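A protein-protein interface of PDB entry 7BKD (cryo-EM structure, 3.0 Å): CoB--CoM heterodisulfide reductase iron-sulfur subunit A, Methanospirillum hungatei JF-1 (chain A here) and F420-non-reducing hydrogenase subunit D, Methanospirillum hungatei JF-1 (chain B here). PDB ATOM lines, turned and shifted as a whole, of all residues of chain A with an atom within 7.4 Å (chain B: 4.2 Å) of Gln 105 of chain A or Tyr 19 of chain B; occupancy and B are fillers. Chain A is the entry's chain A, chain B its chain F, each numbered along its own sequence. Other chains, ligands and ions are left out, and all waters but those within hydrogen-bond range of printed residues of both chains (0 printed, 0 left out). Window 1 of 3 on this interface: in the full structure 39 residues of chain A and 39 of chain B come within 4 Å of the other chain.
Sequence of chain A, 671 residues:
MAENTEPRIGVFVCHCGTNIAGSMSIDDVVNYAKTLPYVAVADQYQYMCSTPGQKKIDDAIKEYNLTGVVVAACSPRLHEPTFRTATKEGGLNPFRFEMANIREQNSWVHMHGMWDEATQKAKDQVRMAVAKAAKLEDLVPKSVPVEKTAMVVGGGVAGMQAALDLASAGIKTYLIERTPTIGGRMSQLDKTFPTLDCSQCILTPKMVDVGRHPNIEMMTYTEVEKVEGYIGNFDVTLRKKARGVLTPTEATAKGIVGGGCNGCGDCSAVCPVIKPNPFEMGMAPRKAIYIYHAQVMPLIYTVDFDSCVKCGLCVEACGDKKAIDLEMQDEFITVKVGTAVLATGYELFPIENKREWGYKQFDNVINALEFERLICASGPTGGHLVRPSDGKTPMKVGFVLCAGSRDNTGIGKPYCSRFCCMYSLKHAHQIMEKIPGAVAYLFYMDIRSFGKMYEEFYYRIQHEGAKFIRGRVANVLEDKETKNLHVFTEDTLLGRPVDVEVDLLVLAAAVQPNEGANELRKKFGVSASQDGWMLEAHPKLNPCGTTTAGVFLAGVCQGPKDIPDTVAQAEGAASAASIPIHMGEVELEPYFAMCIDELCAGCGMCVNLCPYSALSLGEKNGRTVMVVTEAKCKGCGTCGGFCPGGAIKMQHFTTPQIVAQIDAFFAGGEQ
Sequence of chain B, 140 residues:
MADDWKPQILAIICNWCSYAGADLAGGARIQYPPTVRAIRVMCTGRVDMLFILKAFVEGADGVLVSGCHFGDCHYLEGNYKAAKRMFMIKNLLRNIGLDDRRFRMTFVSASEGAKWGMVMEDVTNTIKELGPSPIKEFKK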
ATOM      1  N   MET A  24     -34.266  -8.645 -16.643  1.00  0.00           N
ATOM      2  CA  MET A  24     -33.488  -9.086 -15.498  1.00  0.00           C
ATOM      3  C   MET A  24     -34.323  -8.928 -14.239  1.00  0.00           C
ATOM      4  O   MET A  24     -35.326  -8.213 -14.223  1.00  0.00           O
ATOM      5  CB  MET A  24     -32.183  -8.299 -15.371  1.00  0.00           C
ATOM      6  CG  MET A  24     -32.387  -6.845 -15.021  1.00  0.00           C
ATOM      7  SD  MET A  24     -30.864  -5.894 -15.058  1.00  0.00           S
ATOM      8  CE  MET A  24     -30.620  -5.722 -16.817  1.00  0.00           C
ATOM      9  N   ALA A  73     -28.716   2.408 -14.003  1.00  0.00           N
ATOM     10  CA  ALA A  73     -29.688   2.967 -14.932  1.00  0.00           C
ATOM     11  C   ALA A  73     -29.065   2.992 -16.322  1.00  0.00           C
ATOM     12  O   ALA A  73     -28.148   2.223 -16.622  1.00  0.00           O
ATOM     13  CB  ALA A  73     -30.153   4.352 -14.459  1.00  0.00           C
ATOM     14  N   CYS A  74     -29.582   3.860 -17.180  1.00  0.00           N
ATOM     15  CA  CYS A  74     -29.124   3.979 -18.556  1.00  0.00           C
ATOM     16  C   CYS A  74     -27.708   4.550 -18.594  1.00  0.00           C
ATOM     17  O   CYS A  74     -27.058   4.762 -17.568  1.00  0.00           O
ATOM     18  CB  CYS A  74     -30.094   4.849 -19.346  1.00  0.00           C
ATOM     19  SG  CYS A  74     -30.564   6.362 -18.489  1.00  0.00           S
ATOM     20  N   SER A  75     -27.214   4.798 -19.804  1.00  0.00           N
ATOM     21  CA  SER A  75     -25.826   5.184 -19.994  1.00  0.00           C
ATOM     22  C   SER A  75     -25.531   6.527 -19.331  1.00  0.00           C
ATOM     23  O   SER A  75     -26.385   7.416 -19.296  1.00  0.00           O
ATOM     24  CB  SER A  75     -25.502   5.270 -21.480  1.00  0.00           C
ATOM     25  OG  SER A  75     -26.226   6.321 -22.090  1.00  0.00           O
ATOM     26  N   PRO A  76     -24.320   6.697 -18.797  1.00  0.00           N
ATOM     27  CA  PRO A  76     -23.947   7.998 -18.224  1.00  0.00           C
ATOM     28  C   PRO A  76     -24.023   9.146 -19.208  1.00  0.00           C
ATOM     29  O   PRO A  76     -24.336  10.267 -18.799  1.00  0.00           O
ATOM     30  CB  PRO A  76     -22.509   7.762 -17.750  1.00  0.00           C
ATOM     31  CG  PRO A  76     -22.454   6.312 -17.470  1.00  0.00           C
ATOM     32  CD  PRO A  76     -23.318   5.661 -18.505  1.00  0.00           C
ATOM     33  N   ARG A  77     -23.753   8.914 -20.494  1.00  0.00           N
ATOM     34  CA  ARG A  77     -23.839  10.002 -21.461  1.00  0.00           C
ATOM     35  C   ARG A  77     -25.267  10.486 -21.668  1.00  0.00           C
ATOM     36  O   ARG A  77     -25.467  11.531 -22.295  1.00  0.00           O
ATOM     37  CB  ARG A  77     -23.246   9.579 -22.800  1.00  0.00           C
ATOM     38  CG  ARG A  77     -21.913   8.877 -22.698  1.00  0.00           C
ATOM     39  CD  ARG A  77     -21.495   8.343 -24.052  1.00  0.00           C
ATOM     40  NE  ARG A  77     -20.693   9.316 -24.783  1.00  0.00           N
ATOM     41  CZ  ARG A  77     -20.960   9.721 -26.017  1.00  0.00           C
ATOM     42  NH1 ARG A  77     -22.015   9.238 -26.658  1.00  0.00           N
ATOM     43  NH2 ARG A  77     -20.178  10.612 -26.608  1.00  0.00           N
ATOM     44  N   MET A  99     -22.385   5.675 -11.943  1.00  0.00           N
ATOM     45  CA  MET A  99     -23.499   5.120 -12.693  1.00  0.00           C
ATOM     46  C   MET A  99     -23.126   3.763 -13.267  1.00  0.00           C
ATOM     47  O   MET A  99     -21.988   3.550 -13.693  1.00  0.00           O
ATOM     48  CB  MET A  99     -23.915   6.067 -13.818  1.00  0.00           C
ATOM     49  CG  MET A  99     -25.329   5.856 -14.317  1.00  0.00           C
ATOM     50  SD  MET A  99     -25.958   7.311 -15.166  1.00  0.00           S
ATOM     51  CE  MET A  99     -27.700   6.931 -15.215  1.00  0.00           C
ATOM     52  N   ALA A 100     -24.092   2.851 -13.277  1.00  0.00           N
ATOM     53  CA  ALA A 100     -23.937   1.521 -13.858  1.00  0.00           C
ATOM     54  C   ALA A 100     -24.901   1.399 -15.029  1.00  0.00           C
ATOM     55  O   ALA A 100     -26.121   1.415 -14.841  1.00  0.00           O
ATOM     56  CB  ALA A 100     -24.198   0.435 -12.820  1.00  0.00           C
ATOM     57  N   ASN A 101     -24.355   1.269 -16.233  1.00  0.00           N
ATOM     58  CA  ASN A 101     -25.156   1.151 -17.449  1.00  0.00           C
ATOM     59  C   ASN A 101     -25.743  -0.252 -17.524  1.00  0.00           C
ATOM     60  O   ASN A 101     -25.065  -1.199 -17.921  1.00  0.00           O
ATOM     61  CB  ASN A 101     -24.292   1.455 -18.667  1.00  0.00           C
ATOM     62  CG  ASN A 101     -25.098   1.620 -19.935  1.00  0.00           C
ATOM     63  OD1 ASN A 101     -26.259   1.236 -20.001  1.00  0.00           O
ATOM     64  ND2 ASN A 101     -24.477   2.192 -20.954  1.00  0.00           N
ATOM     65  N   ILE A 102     -27.012  -0.399 -17.148  1.00  0.00           N
ATOM     66  CA  ILE A 102     -27.664  -1.699 -17.168  1.00  0.00           C
ATOM     67  C   ILE A 102     -28.815  -1.753 -18.161  1.00  0.00           C
ATOM     68  O   ILE A 102     -29.599  -2.699 -18.138  1.00  0.00           O
ATOM     69  CB  ILE A 102     -28.140  -2.115 -15.762  1.00  0.00           C
ATOM     70  CG1 ILE A 102     -29.365  -1.312 -15.339  1.00  0.00           C
ATOM     71  CG2 ILE A 102     -27.026  -1.952 -14.753  1.00  0.00           C
ATOM     72  CD1 ILE A 102     -30.102  -1.922 -14.176  1.00  0.00           C
ATOM     73  N   ARG A 103     -28.929  -0.764 -19.045  1.00  0.00           N
ATOM     74  CA  ARG A 103     -29.960  -0.775 -20.074  1.00  0.00           C
ATOM     75  C   ARG A 103     -29.377  -0.867 -21.477  1.00  0.00           C
ATOM     76  O   ARG A 103     -29.688  -1.806 -22.212  1.00  0.00           O
ATOM     77  CB  ARG A 103     -30.842   0.470 -19.951  1.00  0.00           C
ATOM     78  CG  ARG A 103     -32.142   0.371 -20.712  1.00  0.00           C
ATOM     79  CD  ARG A 103     -32.816   1.717 -20.792  1.00  0.00           C
ATOM     80  NE  ARG A 103     -32.035   2.662 -21.576  1.00  0.00           N
ATOM     81  CZ  ARG A 103     -32.505   3.819 -22.023  1.00  0.00           C
ATOM     82  NH1 ARG A 103     -33.753   4.170 -21.759  1.00  0.00           N
ATOM     83  NH2 ARG A 103     -31.730   4.623 -22.732  1.00  0.00           N
ATOM     84  N   GLU A 104     -28.526   0.078 -21.873  1.00  0.00           N
ATOM     85  CA  GLU A 104     -27.954   0.031 -23.212  1.00  0.00           C
ATOM     86  C   GLU A 104     -26.973  -1.116 -23.383  1.00  0.00           C
ATOM     87  O   GLU A 104     -26.698  -1.512 -24.519  1.00  0.00           O
ATOM     88  CB  GLU A 104     -27.248   1.345 -23.542  1.00  0.00           C
ATOM     89  CG  GLU A 104     -28.127   2.394 -24.183  1.00  0.00           C
ATOM     90  CD  GLU A 104     -28.893   3.211 -23.172  1.00  0.00           C
ATOM     91  OE1 GLU A 104     -28.752   2.944 -21.961  1.00  0.00           O
ATOM     92  OE2 GLU A 104     -29.635   4.124 -23.586  1.00  0.00           O
ATOM     93  N   GLN A 105     -26.437  -1.653 -22.292  1.00  0.00           N
ATOM     94  CA  GLN A 105     -25.404  -2.668 -22.369  1.00  0.00           C
ATOM     95  C   GLN A 105     -25.765  -3.974 -21.687  1.00  0.00           C
ATOM     96  O   GLN A 105     -24.984  -4.925 -21.772  1.00  0.00           O
ATOM     97  CB  GLN A 105     -24.099  -2.139 -21.761  1.00  0.00           C
ATOM     98  CG  GLN A 105     -23.625  -0.855 -22.398  1.00  0.00           C
ATOM     99  CD  GLN A 105     -22.176  -0.567 -22.111  1.00  0.00           C
ATOM    100  OE1 GLN A 105     -21.610  -1.075 -21.146  1.00  0.00           O
ATOM    101  NE2 GLN A 105     -21.561   0.254 -22.949  1.00  0.00           N
ATOM    102  N   ASN A 106     -26.888  -4.051 -21.009  1.00  0.00           N
ATOM    103  CA  ASN A 106     -27.243  -5.305 -20.360  1.00  0.00           C
ATOM    104  C   ASN A 106     -28.659  -5.766 -20.659  1.00  0.00           C
ATOM    105  O   ASN A 106     -28.883  -6.963 -20.838  1.00  0.00           O
ATOM    106  CB  ASN A 106     -27.055  -5.165 -18.855  1.00  0.00           C
ATOM    107  CG  ASN A 106     -27.150  -6.484 -18.132  1.00  0.00           C
ATOM    108  OD1 ASN A 106     -27.310  -7.536 -18.741  1.00  0.00           O
ATOM    109  ND2 ASN A 106     -27.054  -6.433 -16.820  1.00  0.00           N
ATOM    110  N   SER A 107     -29.621  -4.855 -20.726  1.00  0.00           N
ATOM    111  CA  SER A 107     -31.017  -5.257 -20.819  1.00  0.00           C
ATOM    112  C   SER A 107     -31.556  -5.239 -22.236  1.00  0.00           C
ATOM    113  O   SER A 107     -32.414  -6.060 -22.569  1.00  0.00           O
ATOM    114  CB  SER A 107     -31.889  -4.353 -19.947  1.00  0.00           C
ATOM    115  OG  SER A 107     -33.239  -4.768 -20.000  1.00  0.00           O
ATOM    116  N   TRP A 108     -31.080  -4.328 -23.073  1.00  0.00           N
ATOM    117  CA  TRP A 108     -31.552  -4.231 -24.442  1.00  0.00           C
ATOM    118  C   TRP A 108     -30.791  -5.135 -25.399  1.00  0.00           C
ATOM    119  O   TRP A 108     -31.198  -5.264 -26.556  1.00  0.00           O
ATOM    120  CB  TRP A 108     -31.455  -2.787 -24.923  1.00  0.00           C
ATOM    121  CG  TRP A 108     -32.595  -1.947 -24.477  1.00  0.00           C
ATOM    122  CD1 TRP A 108     -33.701  -2.363 -23.805  1.00  0.00           C
ATOM    123  CD2 TRP A 108     -32.746  -0.541 -24.672  1.00  0.00           C
ATOM    124  NE1 TRP A 108     -34.535  -1.302 -23.569  1.00  0.00           N
ATOM    125  CE2 TRP A 108     -33.969  -0.170 -24.093  1.00  0.00           C
ATOM    126  CE3 TRP A 108     -31.965   0.440 -25.282  1.00  0.00           C
ATOM    127  CZ2 TRP A 108     -34.430   1.138 -24.106  1.00  0.00           C
ATOM    128  CZ3 TRP A 108     -32.422   1.733 -25.295  1.00  0.00           C
ATOM    129  CH2 TRP A 108     -33.643   2.074 -24.712  1.00  0.00           C
ATOM    130  N   VAL A 109     -29.704  -5.755 -24.950  1.00  0.00           N
ATOM    131  CA  VAL A 109     -28.917  -6.654 -25.783  1.00  0.00           C
ATOM    132  C   VAL A 109     -28.964  -8.086 -25.293  1.00  0.00           C
ATOM    133  O   VAL A 109     -28.357  -8.960 -25.921  1.00  0.00           O
ATOM    134  CB  VAL A 109     -27.460  -6.175 -25.900  1.00  0.00           C
ATOM    135  CG1 VAL A 109     -27.406  -4.821 -26.559  1.00  0.00           C
ATOM    136  CG2 VAL A 109     -26.824  -6.106 -24.536  1.00  0.00           C
ATOM    137  N   HIS A 110     -29.659  -8.359 -24.194  1.00  0.00           N
ATOM    138  CA  HIS A 110     -29.792  -9.705 -23.650  1.00  0.00           C
ATOM    139  C   HIS A 110     -31.252 -10.018 -23.368  1.00  0.00           C
ATOM    140  O   HIS A 110     -31.613 -10.504 -22.296  1.00  0.00           O
ATOM    141  CB  HIS A 110     -28.964  -9.885 -22.382  1.00  0.00           C
ATOM    142  CG  HIS A 110     -27.543  -9.433 -22.509  1.00  0.00           C
ATOM    143  ND1 HIS A 110     -26.816  -9.575 -23.668  1.00  0.00           N
ATOM    144  CD2 HIS A 110     -26.713  -8.848 -21.615  1.00  0.00           C
ATOM    145  CE1 HIS A 110     -25.602  -9.092 -23.486  1.00  0.00           C
ATOM    146  NE2 HIS A 110     -25.514  -8.642 -22.249  1.00  0.00           N
ATOM    147  N   LYS A 121     -24.898 -10.438 -14.997  1.00  0.00           N
ATOM    148  CA  LYS A 121     -24.138  -9.322 -15.547  1.00  0.00           C
ATOM    149  C   LYS A 121     -24.499  -8.017 -14.854  1.00  0.00           C
ATOM    150  O   LYS A 121     -23.632  -7.165 -14.631  1.00  0.00           O
ATOM    151  CB  LYS A 121     -24.374  -9.213 -17.051  1.00  0.00           C
ATOM    152  CG  LYS A 121     -23.666  -8.041 -17.697  1.00  0.00           C
ATOM    153  CD  LYS A 121     -23.601  -8.197 -19.196  1.00  0.00           C
ATOM    154  CE  LYS A 121     -23.148  -6.917 -19.852  1.00  0.00           C
ATOM    155  NZ  LYS A 121     -22.685  -7.151 -21.241  1.00  0.00           N
ATOM    156  N   GLN A 125     -21.960  -5.537 -12.916  1.00  0.00           N
ATOM    157  CA  GLN A 125     -21.854  -4.115 -13.223  1.00  0.00           C
ATOM    158  C   GLN A 125     -22.074  -3.261 -11.984  1.00  0.00           C
ATOM    159  O   GLN A 125     -21.343  -2.290 -11.752  1.00  0.00           O
ATOM    160  CB  GLN A 125     -22.854  -3.739 -14.311  1.00  0.00           C
ATOM    161  CG  GLN A 125     -22.545  -4.325 -15.668  1.00  0.00           C
ATOM    162  CD  GLN A 125     -23.429  -3.757 -16.752  1.00  0.00           C
ATOM    163  OE1 GLN A 125     -24.595  -4.118 -16.869  1.00  0.00           O
ATOM    164  NE2 GLN A 125     -22.876  -2.859 -17.552  1.00  0.00           N
ATOM    165  N   ILE B  13     -13.074   0.284 -22.682  1.00  0.00           N
ATOM    166  CA  ILE B  13     -13.508   0.962 -23.895  1.00  0.00           C
ATOM    167  C   ILE B  13     -13.551   2.461 -23.642  1.00  0.00           C
ATOM    168  O   ILE B  13     -13.965   2.905 -22.568  1.00  0.00           O
ATOM    169  CB  ILE B  13     -14.879   0.441 -24.364  1.00  0.00           C
ATOM    170  CG1 ILE B  13     -15.914   0.570 -23.256  1.00  0.00           C
ATOM    171  CG2 ILE B  13     -14.776  -1.005 -24.771  1.00  0.00           C
ATOM    172  CD1 ILE B  13     -17.240  -0.031 -23.615  1.00  0.00           C
ATOM    173  N   CYS B  14     -13.110   3.237 -24.626  1.00  0.00           N
ATOM    174  CA  CYS B  14     -13.063   4.680 -24.462  1.00  0.00           C
ATOM    175  C   CYS B  14     -14.471   5.264 -24.461  1.00  0.00           C
ATOM    176  O   CYS B  14     -15.417   4.685 -24.996  1.00  0.00           O
ATOM    177  CB  CYS B  14     -12.213   5.326 -25.559  1.00  0.00           C
ATOM    178  SG  CYS B  14     -13.021   5.629 -27.134  1.00  0.00           S
ATOM    179  N   ASN B  15     -14.602   6.427 -23.824  1.00  0.00           N
ATOM    180  CA  ASN B  15     -15.912   7.049 -23.672  1.00  0.00           C
ATOM    181  C   ASN B  15     -16.501   7.471 -25.009  1.00  0.00           C
ATOM    182  O   ASN B  15     -17.698   7.294 -25.248  1.00  0.00           O
ATOM    183  CB  ASN B  15     -15.810   8.257 -22.749  1.00  0.00           C
ATOM    184  CG  ASN B  15     -17.134   8.954 -22.559  1.00  0.00           C
ATOM    185  OD1 ASN B  15     -18.189   8.332 -22.618  1.00  0.00           O
ATOM    186  ND2 ASN B  15     -17.087  10.259 -22.357  1.00  0.00           N
ATOM    187  N   CYS B  17     -15.914   6.896 -28.493  1.00  0.00           N
ATOM    188  CA  CYS B  17     -16.263   6.092 -29.658  1.00  0.00           C
ATOM    189  C   CYS B  17     -16.770   4.708 -29.299  1.00  0.00           C
ATOM    190  O   CYS B  17     -17.871   4.333 -29.714  1.00  0.00           O
ATOM    191  CB  CYS B  17     -15.063   5.970 -30.604  1.00  0.00           C
ATOM    192  SG  CYS B  17     -14.895   7.336 -31.771  1.00  0.00           S
ATOM    193  N   SER B  18     -16.000   3.929 -28.543  1.00  0.00           N
ATOM    194  CA  SER B  18     -16.402   2.555 -28.268  1.00  0.00           C
ATOM    195  C   SER B  18     -17.626   2.500 -27.367  1.00  0.00           C
ATOM    196  O   SER B  18     -18.532   1.689 -27.590  1.00  0.00           O
ATOM    197  CB  SER B  18     -15.241   1.790 -27.646  1.00  0.00           C
ATOM    198  OG  SER B  18     -14.165   1.702 -28.558  1.00  0.00           O
ATOM    199  N   TYR B  19     -17.671   3.349 -26.341  1.00  0.00           N
ATOM    200  CA  TYR B  19     -18.833   3.375 -25.463  1.00  0.00           C
ATOM    201  C   TYR B  19     -20.063   3.872 -26.207  1.00  0.00           C
ATOM    202  O   TYR B  19     -21.167   3.342 -26.028  1.00  0.00           O
ATOM    203  CB  TYR B  19     -18.544   4.247 -24.246  1.00  0.00           C
ATOM    204  CG  TYR B  19     -19.357   3.883 -23.032  1.00  0.00           C
ATOM    205  CD1 TYR B  19     -20.475   4.612 -22.677  1.00  0.00           C
ATOM    206  CD2 TYR B  19     -19.003   2.804 -22.242  1.00  0.00           C
ATOM    207  CE1 TYR B  19     -21.215   4.281 -21.572  1.00  0.00           C
ATOM    208  CE2 TYR B  19     -19.736   2.464 -21.137  1.00  0.00           C
ATOM    209  CZ  TYR B  19     -20.841   3.206 -20.806  1.00  0.00           C
ATOM    210  OH  TYR B  19     -21.576   2.868 -19.698  1.00  0.00           O
ATOM    211  N   ALA B  20     -19.888   4.883 -27.058  1.00  0.00           N
ATOM    212  CA  ALA B  20     -20.990   5.343 -27.890  1.00  0.00           C
ATOM    213  C   ALA B  20     -21.450   4.249 -28.841  1.00  0.00           C
ATOM    214  O   ALA B  20     -22.651   4.095 -29.087  1.00  0.00           O
ATOM    215  CB  ALA B  20     -20.573   6.587 -28.669  1.00  0.00           C
ATOM    216  N   GLY B  21     -20.508   3.482 -29.391  1.00  0.00           N
ATOM    217  CA  GLY B  21     -20.882   2.378 -30.258  1.00  0.00           C
ATOM    218  C   GLY B  21     -21.676   1.308 -29.537  1.00  0.00           C
ATOM    219  O   GLY B  21     -22.650   0.778 -30.073  1.00  0.00           O
ATOM    220  N   ALA B  22     -21.270   0.971 -28.313  1.00  0.00           N
ATOM    221  CA  ALA B  22     -22.030   0.000 -27.532  1.00  0.00           C
ATOM    222  C   ALA B  22     -23.419   0.531 -27.196  1.00  0.00           C
ATOM    223  O   ALA B  22     -24.405  -0.217 -27.225  1.00  0.00           O
ATOM    224  CB  ALA B  22     -21.269  -0.362 -26.260  1.00  0.00           C
ATOM    225  N   ASP B  23     -23.516   1.822 -26.874  1.00  0.00           N
ATOM    226  CA  ASP B  23     -24.820   2.424 -26.623  1.00  0.00           C
ATOM    227  C   ASP B  23     -25.704   2.352 -27.860  1.00  0.00           C
ATOM    228  O   ASP B  23     -26.899   2.057 -27.763  1.00  0.00           O
ATOM    229  CB  ASP B  23     -24.650   3.875 -26.178  1.00  0.00           C
ATOM    230  CG  ASP B  23     -24.040   3.995 -24.801  1.00  0.00           C
ATOM    231  OD1 ASP B  23     -23.749   2.950 -24.186  1.00  0.00           O
ATOM    232  OD2 ASP B  23     -23.848   5.137 -24.335  1.00  0.00           O
ATOM    233  N   TYR B  32     -26.197  -9.955 -28.449  1.00  0.00           N
ATOM    234  CA  TYR B  32     -24.914 -10.635 -28.358  1.00  0.00           C
ATOM    235  C   TYR B  32     -24.798 -11.258 -26.974  1.00  0.00           C
ATOM    236  O   TYR B  32     -25.486 -10.831 -26.043  1.00  0.00           O
ATOM    237  CB  TYR B  32     -23.745  -9.679 -28.646  1.00  0.00           C
ATOM    238  CG  TYR B  32     -23.642  -8.440 -27.790  1.00  0.00           C
ATOM    239  CD1 TYR B  32     -23.150  -8.503 -26.499  1.00  0.00           C
ATOM    240  CD2 TYR B  32     -23.979  -7.198 -28.298  1.00  0.00           C
ATOM    241  CE1 TYR B  32     -23.029  -7.370 -25.727  1.00  0.00           C
ATOM    242  CE2 TYR B  32     -23.860  -6.062 -27.535  1.00  0.00           C
ATOM    243  CZ  TYR B  32     -23.385  -6.154 -26.249  1.00  0.00           C
ATOM    244  OH  TYR B  32     -23.263  -5.023 -25.480  1.00  0.00           O
ATOM    245  N   ARG B  40     -14.875   1.722 -19.234  1.00  0.00           N
ATOM    246  CA  ARG B  40     -15.181   3.096 -19.642  1.00  0.00           C
ATOM    247  C   ARG B  40     -14.172   4.102 -19.074  1.00  0.00           C
ATOM    248  O   ARG B  40     -14.461   4.893 -18.178  1.00  0.00           O
ATOM    249  CB  ARG B  40     -16.615   3.473 -19.255  1.00  0.00           C
ATOM    250  CG  ARG B  40     -17.059   4.830 -19.758  1.00  0.00           C
ATOM    251  CD  ARG B  40     -17.971   5.492 -18.754  1.00  0.00           C
ATOM    252  NE  ARG B  40     -18.426   6.796 -19.214  1.00  0.00           N
ATOM    253  CZ  ARG B  40     -18.404   7.892 -18.468  1.00  0.00           C
ATOM    254  NH1 ARG B  40     -17.952   7.837 -17.226  1.00  0.00           N
ATOM    255  NH2 ARG B  40     -18.834   9.042 -18.964  1.00  0.00           N
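The backbone carbonyl oxygen of Tyr 32 of chain B lies within hydrogen-bond range of a ring nitrogen (ND1) of His 110 of chain A, at 3.0 Å. O of Val 109 of chain A sits at hydrogen-bond distance from N of Tyr 32 of chain B, at 3.5 Å. The side-chain amide nitrogen (ND2) of Asn 101 of chain A is in hydrogen-bond range of the side-chain carboxylate (OD1) of Asp 23 of chain B, at 3.4 Å. NE of Arg 77 of chain A lies within hydrogen-bond range of OD1 of Asn 15 of chain B. OD2 of Asp 23 of chain B lies close to OG of Ser 75 of chain A (3.5 Å). The side-chain amide nitrogen of Asn 101 of chain A sits close to the side-chain hydroxyl of Tyr 19 of chain B (3.2 Å).
The side-chain carboxylate (OE1) of Glu 104 of chain A lies within salt-bridge range of the guanidinium group (NE) of Arg 103 of chain A (3.3 Å). NE2 of Gln 125 of chain A lies within hydrogen-bond range of O of Asn 101 of chain A (2.8 Å). N of Glu 104 of chain A is in hydrogen-bond range of OD1 of Asn 101 of chain A. O of Cys 14 of chain B is in hydrogen-bond range of N of Tyr 19 of chain B, 2.9 Å away. The side-chain amino group (NZ) of Lys 121 of chain A lies within hydrogen-bond range of a ring nitrogen (NE2) of His 110 of chain A, 3.4 Å away. OD1 of Asn 101 of chain A sits at hydrogen-bond distance from N of Arg 103 of chain A (3.5 Å).
Among the printed residues, pairs that only touch across the chains: Gln 105 of chain A with Ala 22 of chain B (3.4 Å), Gln 105 of chain A with Tyr 19 of chain B (3.4 Å), Pro 76 of chain A with Tyr 19 of chain B (3.5 Å), Arg 77 of chain A with Ala 20 of chain B (3.6 Å), Gln 105 of chain A with Asp 23 of chain B (3.7 Å), Glu 104 of chain A with Ala 22 of chain B (3.8 Å), Glu 104 of chain A with Asp 23 of chain B (3.8 Å) and Arg 77 of chain A with Asp 23 of chain B (3.99 Å).
Cys 74 of chain A touches none of the printed residues of chain B. Of the printed residues of chain B, Glu 104 of chain A touches Ala 22 (3.8 Å) and Asp 23 (3.8 Å). Gln 105 of chain A touches just these residues of chain B: Tyr 19 (3.4 Å), Ala 22 (3.4 Å) and Asp 23 (3.7 Å). Trp 108 of chain A touches none of the printed residues of chain B. Of the printed residues of chain B, His 110 of chain A touches Tyr 32. Of the printed residues of chain A, Tyr 19 of chain B touches Pro 76, Asn 101 and Gln 105. Of the printed residues of chain A, Asp 23 of chain B touches Ser 75, Arg 77, Asn 101, Glu 104 and Gln 105. Of the printed residues of chain A, Tyr 32 of chain B touches Val 109 and His 110. The nearest residue of chain A that does not touch Tyr 19 of chain B is Arg 77 of chain A (4.1 Å). The nearest printed residue of chain B that does not touch Asn 101 of chain A is Ala 22 of chain B (6.5 Å).
Of the 20 printed residues of chain A, 8 touch a printed residue of chain B. Of the 12 printed residues of chain B, 6 touch a printed residue of chain A. Hydrophobic or aromatic side chains of chain B within 4 Å of the printed part of chain A: Tyr 19, Ala 20, Ala 22 and Tyr 32. Among the printed residues, 14 pairs touch across the chains.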
